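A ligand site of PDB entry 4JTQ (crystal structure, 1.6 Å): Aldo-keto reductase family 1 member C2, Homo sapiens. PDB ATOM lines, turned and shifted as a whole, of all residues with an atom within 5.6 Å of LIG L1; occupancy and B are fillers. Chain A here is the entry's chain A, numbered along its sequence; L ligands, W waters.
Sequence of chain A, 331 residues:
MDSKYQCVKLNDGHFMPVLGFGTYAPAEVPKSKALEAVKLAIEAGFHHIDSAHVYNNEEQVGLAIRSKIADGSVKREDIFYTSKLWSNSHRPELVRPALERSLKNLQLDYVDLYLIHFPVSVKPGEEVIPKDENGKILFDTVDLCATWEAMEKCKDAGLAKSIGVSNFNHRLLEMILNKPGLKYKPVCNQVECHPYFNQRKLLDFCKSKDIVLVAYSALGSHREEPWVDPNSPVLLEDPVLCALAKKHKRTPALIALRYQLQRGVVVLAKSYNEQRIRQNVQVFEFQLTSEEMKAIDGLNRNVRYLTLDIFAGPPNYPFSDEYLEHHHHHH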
ATOM      1  N   TYR A  24      10.437   9.167  21.704  1.00  0.00           N
ATOM      2  CA  TYR A  24       9.389   9.974  21.076  1.00  0.00           C
ATOM      3  C   TYR A  24       9.662  10.121  19.581  1.00  0.00           C
ATOM      4  O   TYR A  24      10.791  10.305  19.161  1.00  0.00           O
ATOM      5  CB  TYR A  24       9.349  11.371  21.651  1.00  0.00           C
ATOM      6  CG  TYR A  24       8.270  12.169  20.999  1.00  0.00           C
ATOM      7  CD1 TYR A  24       6.912  11.909  21.250  1.00  0.00           C
ATOM      8  CD2 TYR A  24       8.578  13.122  20.054  1.00  0.00           C
ATOM      9  CE1 TYR A  24       5.916  12.626  20.589  1.00  0.00           C
ATOM     10  CE2 TYR A  24       7.600  13.817  19.363  1.00  0.00           C
ATOM     11  CZ  TYR A  24       6.260  13.565  19.625  1.00  0.00           C
ATOM     12  OH  TYR A  24       5.262  14.266  18.978  1.00  0.00           O
ATOM     13  N   ALA A  52       7.050   7.750  27.987  1.00  0.00           N
ATOM     14  CA  ALA A  52       6.000   8.600  28.585  1.00  0.00           C
ATOM     15  C   ALA A  52       4.652   8.148  28.100  1.00  0.00           C
ATOM     16  O   ALA A  52       4.463   7.750  26.948  1.00  0.00           O
ATOM     17  CB  ALA A  52       6.159  10.062  28.215  1.00  0.00           C
ATOM     18  N   VAL A  54       2.270  10.171  27.194  1.00  0.00           N
ATOM     19  CA  VAL A  54       1.842  11.052  26.078  1.00  0.00           C
ATOM     20  C   VAL A  54       2.480  10.702  24.724  1.00  0.00           C
ATOM     21  O   VAL A  54       2.032  11.175  23.671  1.00  0.00           O
ATOM     22  CB  VAL A  54       2.059  12.535  26.562  1.00  0.00           C
ATOM     23  CG1 VAL A  54       3.509  12.957  26.496  1.00  0.00           C
ATOM     24  CG2 VAL A  54       1.105  13.491  25.940  1.00  0.00           C
ATOM     25  N   TYR A  55       3.578   9.929  24.754  1.00  0.00           N
ATOM     26  CA  TYR A  55       4.238   9.496  23.503  1.00  0.00           C
ATOM     27  C   TYR A  55       3.418   8.474  22.733  1.00  0.00           C
ATOM     28  O   TYR A  55       3.674   8.254  21.545  1.00  0.00           O
ATOM     29  CB  TYR A  55       5.641   8.925  23.766  1.00  0.00           C
ATOM     30  CG  TYR A  55       6.633   9.875  24.404  1.00  0.00           C
ATOM     31  CD1 TYR A  55       6.327  11.204  24.584  1.00  0.00           C
ATOM     32  CD2 TYR A  55       7.847   9.419  24.898  1.00  0.00           C
ATOM     33  CE1 TYR A  55       7.207  12.073  25.217  1.00  0.00           C
ATOM     34  CE2 TYR A  55       8.739  10.277  25.520  1.00  0.00           C
ATOM     35  CZ  TYR A  55       8.416  11.593  25.731  1.00  0.00           C
ATOM     36  OH  TYR A  55       9.280  12.458  26.366  1.00  0.00           O
ATOM     37  N   LYS A  84       6.486   8.738  32.412  1.00  0.00           N
ATOM     38  CA  LYS A  84       6.163  10.026  32.898  1.00  0.00           C
ATOM     39  C   LYS A  84       4.650  10.147  33.031  1.00  0.00           C
ATOM     40  O   LYS A  84       3.854   9.696  32.164  1.00  0.00           O
ATOM     41  CB  LYS A  84       6.711  11.142  31.959  1.00  0.00           C
ATOM     42  CG  LYS A  84       8.126  10.918  31.452  1.00  0.00           C
ATOM     43  CD  LYS A  84       8.742  12.137  30.751  1.00  0.00           C
ATOM     44  CE  LYS A  84      10.134  11.787  30.184  1.00  0.00           C
ATOM     45  NZ  LYS A  84      10.022  11.053  28.881  1.00  0.00           N
ATOM     46  N   TRP A  86       1.502  12.253  32.847  1.00  0.00           N
ATOM     47  CA  TRP A  86       1.004  13.341  32.001  1.00  0.00           C
ATOM     48  C   TRP A  86       0.106  14.259  32.853  1.00  0.00           C
ATOM     49  O   TRP A  86      -0.418  13.881  33.900  1.00  0.00           O
ATOM     50  CB  TRP A  86       0.301  12.842  30.716  1.00  0.00           C
ATOM     51  CG  TRP A  86       0.025  14.055  29.825  1.00  0.00           C
ATOM     52  CD1 TRP A  86      -1.218  14.534  29.453  1.00  0.00           C
ATOM     53  CD2 TRP A  86       0.975  15.049  29.402  1.00  0.00           C
ATOM     54  NE1 TRP A  86      -1.078  15.710  28.761  1.00  0.00           N
ATOM     55  CE2 TRP A  86       0.263  16.053  28.746  1.00  0.00           C
ATOM     56  CE3 TRP A  86       2.372  15.182  29.513  1.00  0.00           C
ATOM     57  CZ2 TRP A  86       0.909  17.170  28.195  1.00  0.00           C
ATOM     58  CZ3 TRP A  86       3.002  16.296  28.965  1.00  0.00           C
ATOM     59  CH2 TRP A  86       2.265  17.255  28.290  1.00  0.00           C
ATOM     60  N   HIS A 117       5.806  14.923  34.291  1.00  0.00           N
ATOM     61  CA  HIS A 117       6.256  15.298  32.901  1.00  0.00           C
ATOM     62  C   HIS A 117       6.373  16.803  32.709  1.00  0.00           C
ATOM     63  O   HIS A 117       7.349  17.277  32.156  1.00  0.00           O
ATOM     64  CB  HIS A 117       5.330  14.676  31.870  1.00  0.00           C
ATOM     65  CG  HIS A 117       5.933  14.531  30.505  1.00  0.00           C
ATOM     66  ND1 HIS A 117       5.500  13.566  29.616  1.00  0.00           N
ATOM     67  CD2 HIS A 117       6.943  15.212  29.891  1.00  0.00           C
ATOM     68  CE1 HIS A 117       6.168  13.694  28.491  1.00  0.00           C
ATOM     69  NE2 HIS A 117       7.074  14.665  28.646  1.00  0.00           N
ATOM     70  N   VAL A 128      -5.351  13.877  26.278  1.00  0.00           N
ATOM     71  CA  VAL A 128      -4.104  14.416  26.816  1.00  0.00           C
ATOM     72  C   VAL A 128      -3.995  15.954  26.740  1.00  0.00           C
ATOM     73  O   VAL A 128      -3.314  16.564  27.592  1.00  0.00           O
ATOM     74  CB  VAL A 128      -2.870  13.702  26.209  1.00  0.00           C
ATOM     75  CG1 VAL A 128      -2.875  12.205  26.638  1.00  0.00           C
ATOM     76  CG2 VAL A 128      -2.824  13.866  24.721  1.00  0.00           C
ATOM     77  N   ILE A 129      -4.594  16.553  25.720  1.00  0.00           N
ATOM     78  CA  ILE A 129      -4.682  18.053  25.666  1.00  0.00           C
ATOM     79  C   ILE A 129      -6.153  18.405  25.510  1.00  0.00           C
ATOM     80  O   ILE A 129      -6.653  18.654  24.412  1.00  0.00           O
ATOM     81  CB  ILE A 129      -3.807  18.656  24.560  1.00  0.00           C
ATOM     82  CG1 ILE A 129      -2.311  18.394  24.884  1.00  0.00           C
ATOM     83  CG2 ILE A 129      -4.017  20.164  24.526  1.00  0.00           C
ATOM     84  CD1 ILE A 129      -1.412  18.844  23.813  1.00  0.00           C
ATOM     85  N   ASN A 167      11.122  19.349  33.392  1.00  0.00           N
ATOM     86  CA  ASN A 167      10.679  20.677  32.986  1.00  0.00           C
ATOM     87  C   ASN A 167      10.327  21.548  34.204  1.00  0.00           C
ATOM     88  O   ASN A 167       9.462  22.459  34.145  1.00  0.00           O
ATOM     89  CB  ASN A 167       9.468  20.623  32.025  1.00  0.00           C
ATOM     90  CG  ASN A 167       9.838  19.962  30.707  1.00  0.00           C
ATOM     91  OD1 ASN A 167      10.711  20.446  30.017  1.00  0.00           O
ATOM     92  ND2 ASN A 167       9.187  18.855  30.396  1.00  0.00           N
ATOM     93  N   TYR A 216      17.426  16.283  27.641  1.00  0.00           N
ATOM     94  CA  TYR A 216      16.689  15.968  26.457  1.00  0.00           C
ATOM     95  C   TYR A 216      16.946  16.991  25.353  1.00  0.00           C
ATOM     96  O   TYR A 216      17.511  18.089  25.580  1.00  0.00           O
ATOM     97  CB  TYR A 216      15.231  15.816  26.759  1.00  0.00           C
ATOM     98  CG  TYR A 216      14.392  17.048  26.977  1.00  0.00           C
ATOM     99  CD1 TYR A 216      14.139  17.955  25.970  1.00  0.00           C
ATOM    100  CD2 TYR A 216      13.693  17.190  28.156  1.00  0.00           C
ATOM    101  CE1 TYR A 216      13.223  18.985  26.165  1.00  0.00           C
ATOM    102  CE2 TYR A 216      12.778  18.219  28.350  1.00  0.00           C
ATOM    103  CZ  TYR A 216      12.601  19.149  27.368  1.00  0.00           C
ATOM    104  OH  TYR A 216      11.625  20.117  27.523  1.00  0.00           O
ATOM    105  N   HIS A 222      13.840  16.867  18.002  1.00  0.00           N
ATOM    106  CA  HIS A 222      13.106  16.286  16.871  1.00  0.00           C
ATOM    107  C   HIS A 222      12.697  17.326  15.832  1.00  0.00           C
ATOM    108  O   HIS A 222      12.345  16.998  14.683  1.00  0.00           O
ATOM    109  CB  HIS A 222      11.814  15.584  17.381  1.00  0.00           C
ATOM    110  CG  HIS A 222      11.031  16.368  18.401  1.00  0.00           C
ATOM    111  ND1 HIS A 222      10.349  17.546  18.099  1.00  0.00           N
ATOM    112  CD2 HIS A 222      10.751  16.114  19.711  1.00  0.00           C
ATOM    113  CE1 HIS A 222       9.724  17.992  19.179  1.00  0.00           C
ATOM    114  NE2 HIS A 222       9.948  17.140  20.171  1.00  0.00           N
ATOM    115  N   GLU A 224      10.037  18.898  15.426  1.00  0.00           N
ATOM    116  CA  GLU A 224       8.631  18.772  15.035  1.00  0.00           C
ATOM    117  C   GLU A 224       7.871  20.097  15.121  1.00  0.00           C
ATOM    118  O   GLU A 224       7.882  20.740  16.176  1.00  0.00           O
ATOM    119  CB  GLU A 224       7.939  17.699  15.916  1.00  0.00           C
ATOM    120  CG  GLU A 224       6.641  17.210  15.275  1.00  0.00           C
ATOM    121  CD  GLU A 224       5.817  16.272  16.129  1.00  0.00           C
ATOM    122  OE1 GLU A 224       6.205  15.999  17.291  1.00  0.00           O
ATOM    123  OE2 GLU A 224       4.747  15.823  15.603  1.00  0.00           O
ATOM    124  N   TRP A 227       5.729  22.532  17.544  1.00  0.00           N
ATOM    125  CA  TRP A 227       6.354  22.532  18.866  1.00  0.00           C
ATOM    126  C   TRP A 227       7.708  23.277  18.874  1.00  0.00           C
ATOM    127  O   TRP A 227       8.084  23.964  19.888  1.00  0.00           O
ATOM    128  CB  TRP A 227       6.581  21.085  19.282  1.00  0.00           C
ATOM    129  CG  TRP A 227       5.355  20.309  19.264  1.00  0.00           C
ATOM    130  CD1 TRP A 227       4.925  19.472  18.288  1.00  0.00           C
ATOM    131  CD2 TRP A 227       4.356  20.272  20.315  1.00  0.00           C
ATOM    132  NE1 TRP A 227       3.697  18.913  18.654  1.00  0.00           N
ATOM    133  CE2 TRP A 227       3.337  19.377  19.895  1.00  0.00           C
ATOM    134  CE3 TRP A 227       4.236  20.900  21.563  1.00  0.00           C
ATOM    135  CZ2 TRP A 227       2.188  19.107  20.679  1.00  0.00           C
ATOM    136  CZ3 TRP A 227       3.108  20.641  22.341  1.00  0.00           C
ATOM    137  CH2 TRP A 227       2.111  19.738  21.900  1.00  0.00           C
ATOM    138  N   LEU A 306      12.323  23.808  22.724  1.00  0.00           N
ATOM    139  CA  LEU A 306      10.981  23.347  23.155  1.00  0.00           C
ATOM    140  C   LEU A 306      10.462  24.298  24.240  1.00  0.00           C
ATOM    141  O   LEU A 306      10.757  24.132  25.407  1.00  0.00           O
ATOM    142  CB  LEU A 306      11.162  21.950  23.684  1.00  0.00           C
ATOM    143  CG  LEU A 306      10.238  20.798  23.301  1.00  0.00           C
ATOM    144  CD1 LEU A 306       9.404  20.588  24.541  1.00  0.00           C
ATOM    145  CD2 LEU A 306       9.356  20.904  22.042  1.00  0.00           C
ATOM    146  N   LEU A 308       7.019  24.613  24.693  1.00  0.00           N
ATOM    147  CA  LEU A 308       5.685  24.107  25.089  1.00  0.00           C
ATOM    148  C   LEU A 308       4.740  25.262  25.393  1.00  0.00           C
ATOM    149  O   LEU A 308       3.984  25.202  26.339  1.00  0.00           O
ATOM    150  CB  LEU A 308       5.737  23.115  26.299  1.00  0.00           C
ATOM    151  CG  LEU A 308       6.790  22.027  26.045  1.00  0.00           C
ATOM    152  CD1 LEU A 308       7.249  21.163  27.228  1.00  0.00           C
ATOM    153  CD2 LEU A 308       6.195  21.161  24.937  1.00  0.00           C
ATOM    154  N   ILE A 310       2.060  26.346  24.281  1.00  0.00           N
ATOM    155  CA  ILE A 310       0.611  26.151  24.371  1.00  0.00           C
ATOM    156  C   ILE A 310       0.151  26.009  25.836  1.00  0.00           C
ATOM    157  O   ILE A 310      -1.001  26.268  26.150  1.00  0.00           O
ATOM    158  CB  ILE A 310       0.117  24.985  23.527  1.00  0.00           C
ATOM    159  CG1 ILE A 310       0.623  23.627  24.065  1.00  0.00           C
ATOM    160  CG2 ILE A 310       0.546  25.221  22.076  1.00  0.00           C
ATOM    161  CD1 ILE A 310      -0.053  22.479  23.379  1.00  0.00           C
ATOM    162  N   PHE A 311       1.078  25.690  26.738  1.00  0.00           N
ATOM    163  CA  PHE A 311       0.772  25.626  28.168  1.00  0.00           C
ATOM    164  C   PHE A 311       1.205  26.886  28.943  1.00  0.00           C
ATOM    165  O   PHE A 311       1.173  26.901  30.183  1.00  0.00           O
ATOM    166  CB  PHE A 311       1.457  24.391  28.742  1.00  0.00           C
ATOM    167  CG  PHE A 311       1.109  23.124  28.065  1.00  0.00           C
ATOM    168  CD1 PHE A 311      -0.199  22.626  28.092  1.00  0.00           C
ATOM    169  CD2 PHE A 311       2.130  22.355  27.479  1.00  0.00           C
ATOM    170  CE1 PHE A 311      -0.527  21.414  27.505  1.00  0.00           C
ATOM    171  CE2 PHE A 311       1.819  21.121  26.862  1.00  0.00           C
ATOM    172  CZ  PHE A 311       0.482  20.662  26.890  1.00  0.00           C
HETATM  173  C1  LIG L   1       1.123  15.488  20.107  1.00  0.00           C
HETATM  174  C2  LIG L   1       2.175  15.646  21.024  1.00  0.00           C
HETATM  175  C3  LIG L   1       2.014  15.632  22.454  1.00  0.00           C
HETATM  176  C4  LIG L   1       0.768  15.465  22.997  1.00  0.00           C
HETATM  177  C5  LIG L   1      -0.293  15.316  22.116  1.00  0.00           C
HETATM  178  C6  LIG L   1      -0.145  15.319  20.699  1.00  0.00           C
HETATM  179  C7  LIG L   1       3.147  15.811  23.295  1.00  0.00           C
HETATM  180  C8  LIG L   1       4.312  15.068  23.068  1.00  0.00           C
HETATM  181  C9  LIG L   1       5.434  15.219  23.837  1.00  0.00           C
HETATM  182  C10 LIG L   1       5.424  16.176  24.896  1.00  0.00           C
HETATM  183  C11 LIG L   1       4.282  16.922  25.128  1.00  0.00           C
HETATM  184  C12 LIG L   1       3.181  16.715  24.312  1.00  0.00           C
HETATM  185  C13 LIG L   1       6.558  16.366  25.709  1.00  0.00           C
HETATM  186  C14 LIG L   1       7.096  17.741  25.547  1.00  0.00           C
HETATM  187  C15 LIG L   1       7.833  15.564  25.394  1.00  0.00           C
HETATM  188  O1  LIG L   1       8.272  14.755  26.237  1.00  0.00           O
HETATM  189  O2  LIG L   1       8.273  15.667  24.263  1.00  0.00           O
HETATM  190  F1  LIG L   1       1.994  17.534  24.600  1.00  0.00           F
HETATM  191  P1  LG2 L   2      17.229  14.444  20.134  1.00  0.00           P
HETATM  192  O1  LG2 L   2      17.840  15.759  20.357  1.00  0.00           O
HETATM  193  O2  LG2 L   2      17.743  13.210  20.787  1.00  0.00           O
HETATM  194  O3  LG2 L   2      17.457  14.042  18.603  1.00  0.00           O
HETATM  195  C1  LG2 L   2      17.155  14.751  17.562  1.00  0.00           C
HETATM  196  C2  LG2 L   2      17.392  14.045  16.164  1.00  0.00           C
HETATM  197  O4  LG2 L   2      18.643  13.613  16.074  1.00  0.00           O
HETATM  198  C3  LG2 L   2      16.527  12.824  15.877  1.00  0.00           C
HETATM  199  O5  LG2 L   2      15.602  13.227  15.054  1.00  0.00           O
HETATM  200  C4  LG2 L   2      17.427  11.824  15.160  1.00  0.00           C
HETATM  201  O6  LG2 L   2      17.050  11.380  13.816  1.00  0.00           O
HETATM  202  C5  LG2 L   2      18.730  12.654  15.065  1.00  0.00           C
HETATM  203  N1  LG2 L   2      19.928  11.868  15.427  1.00  0.00           N
HETATM  204  C6  LG2 L   2      20.035  10.921  16.352  1.00  0.00           C
HETATM  205  N2  LG2 L   2      21.312  10.456  16.375  1.00  0.00           N
HETATM  206  C7  LG2 L   2      22.001  11.105  15.432  1.00  0.00           C
HETATM  207  C8  LG2 L   2      23.331  11.067  15.003  1.00  0.00           C
HETATM  208  N3  LG2 L   2      24.209  10.218  15.544  1.00  0.00           N
HETATM  209  N4  LG2 L   2      23.738  11.869  13.994  1.00  0.00           N
HETATM  210  C9  LG2 L   2      22.815  12.710  13.414  1.00  0.00           C
HETATM  211  N5  LG2 L   2      21.501  12.781  13.827  1.00  0.00           N
HETATM  212  C10 LG2 L   2      21.130  11.995  14.857  1.00  0.00           C
HETATM  213  O7  LG2 L   2      15.588  14.308  20.047  1.00  0.00           O
HETATM  214  P2  LG2 L   2      14.445  14.593  21.121  1.00  0.00           P
HETATM  215  O8  LG2 L   2      13.911  15.878  20.995  1.00  0.00           O
HETATM  216  O9  LG2 L   2      13.675  13.473  20.606  1.00  0.00           O
HETATM  217  O10 LG2 L   2      14.977  14.222  22.533  1.00  0.00           O
HETATM  218  C11 LG2 L   2      15.360  12.905  22.899  1.00  0.00           C
HETATM  219  C12 LG2 L   2      14.345  12.284  23.820  1.00  0.00           C
HETATM  220  O11 LG2 L   2      14.245  13.072  25.019  1.00  0.00           O
HETATM  221  C13 LG2 L   2      12.878  12.081  23.280  1.00  0.00           C
HETATM  222  O12 LG2 L   2      12.784  11.011  22.362  1.00  0.00           O
HETATM  223  C14 LG2 L   2      12.142  11.841  24.636  1.00  0.00           C
HETATM  224  O13 LG2 L   2      12.482  10.522  25.082  1.00  0.00           O
HETATM  225  C15 LG2 L   2      12.914  12.855  25.521  1.00  0.00           C
HETATM  226  N6  LG2 L   2      12.272  14.190  25.619  1.00  0.00           N
HETATM  227  C16 LG2 L   2      11.613  14.500  26.815  1.00  0.00           C
HETATM  228  C17 LG2 L   2      11.001  15.724  26.914  1.00  0.00           C
HETATM  229  C18 LG2 L   2      10.340  16.120  28.110  1.00  0.00           C
HETATM  230  O14 LG2 L   2       9.525  17.069  28.210  1.00  0.00           O
HETATM  231  N7  LG2 L   2      10.639  15.449  29.181  1.00  0.00           N
HETATM  232  C19 LG2 L   2      11.078  16.603  25.830  1.00  0.00           C
HETATM  233  C20 LG2 L   2      11.659  16.309  24.640  1.00  0.00           C
HETATM  234  C21 LG2 L   2      12.359  15.133  24.553  1.00  0.00           C
HETATM  235  P3  LG2 L   2      16.963   9.780  13.500  1.00  0.00           P
HETATM  236  O15 LG2 L   2      15.911   9.162  14.414  1.00  0.00           O
HETATM  237  O16 LG2 L   2      16.609   9.799  12.061  1.00  0.00           O
HETATM  238  O17 LG2 L   2      18.369   9.218  13.705  1.00  0.00           O
HETATM  239  O   HOH W   1       9.962  14.103  23.056  1.00  0.00           O
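An oxygen (O14) of LG2 L2 sits at hydrogen-bond distance from a ring nitrogen (NE2) of His 117 (3.5 Å). ND2 of Asn 167 lies within hydrogen-bond range of O14 of LG2 L2, 2.8 Å away. O1 of LIG L1 sits at hydrogen-bond distance from OH of Tyr 55, 2.5 Å away. The backbone NH (N) of His 222 sits at hydrogen-bond distance from an oxygen (O8) of LG2 L2, 3.2 Å away. An oxygen (O12) of LG2 L2 is in hydrogen-bond range of the backbone NH (N) of Tyr 24, 3.1 Å away. A ring nitrogen (NE2) of His 117 sits at hydrogen-bond distance from an oxygen (O1) of LIG L1, 2.7 Å away.
The side-chain carboxylate (OE1) of Glu 224 is in hydrogen-bond range of the side-chain hydroxyl (OH) of Tyr 24 (2.6 Å). O of His 117 is in hydrogen-bond range of ND2 of Asn 167 (3.0 Å). The indole nitrogen of Trp 86 is in hydrogen-bond range of the backbone carbonyl oxygen of Val 128, 2.7 Å away. The side-chain hydroxyl (OH) of Tyr 55 lies within hydrogen-bond range of the side-chain amino group (NZ) of Lys 84, at 3.0 Å.
Residues that only touch LIG L1: Tyr 24, Val 54, Trp 86, Val 128, Ile 129, Trp 227, Leu 306 and Leu 308. Ten residues have an atom within 4 Å of LIG L1: Tyr 24, Val 54, Tyr 55, Trp 86, His 117, Val 128, Ile 129, Trp 227, Leu 306 and Leu 308.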
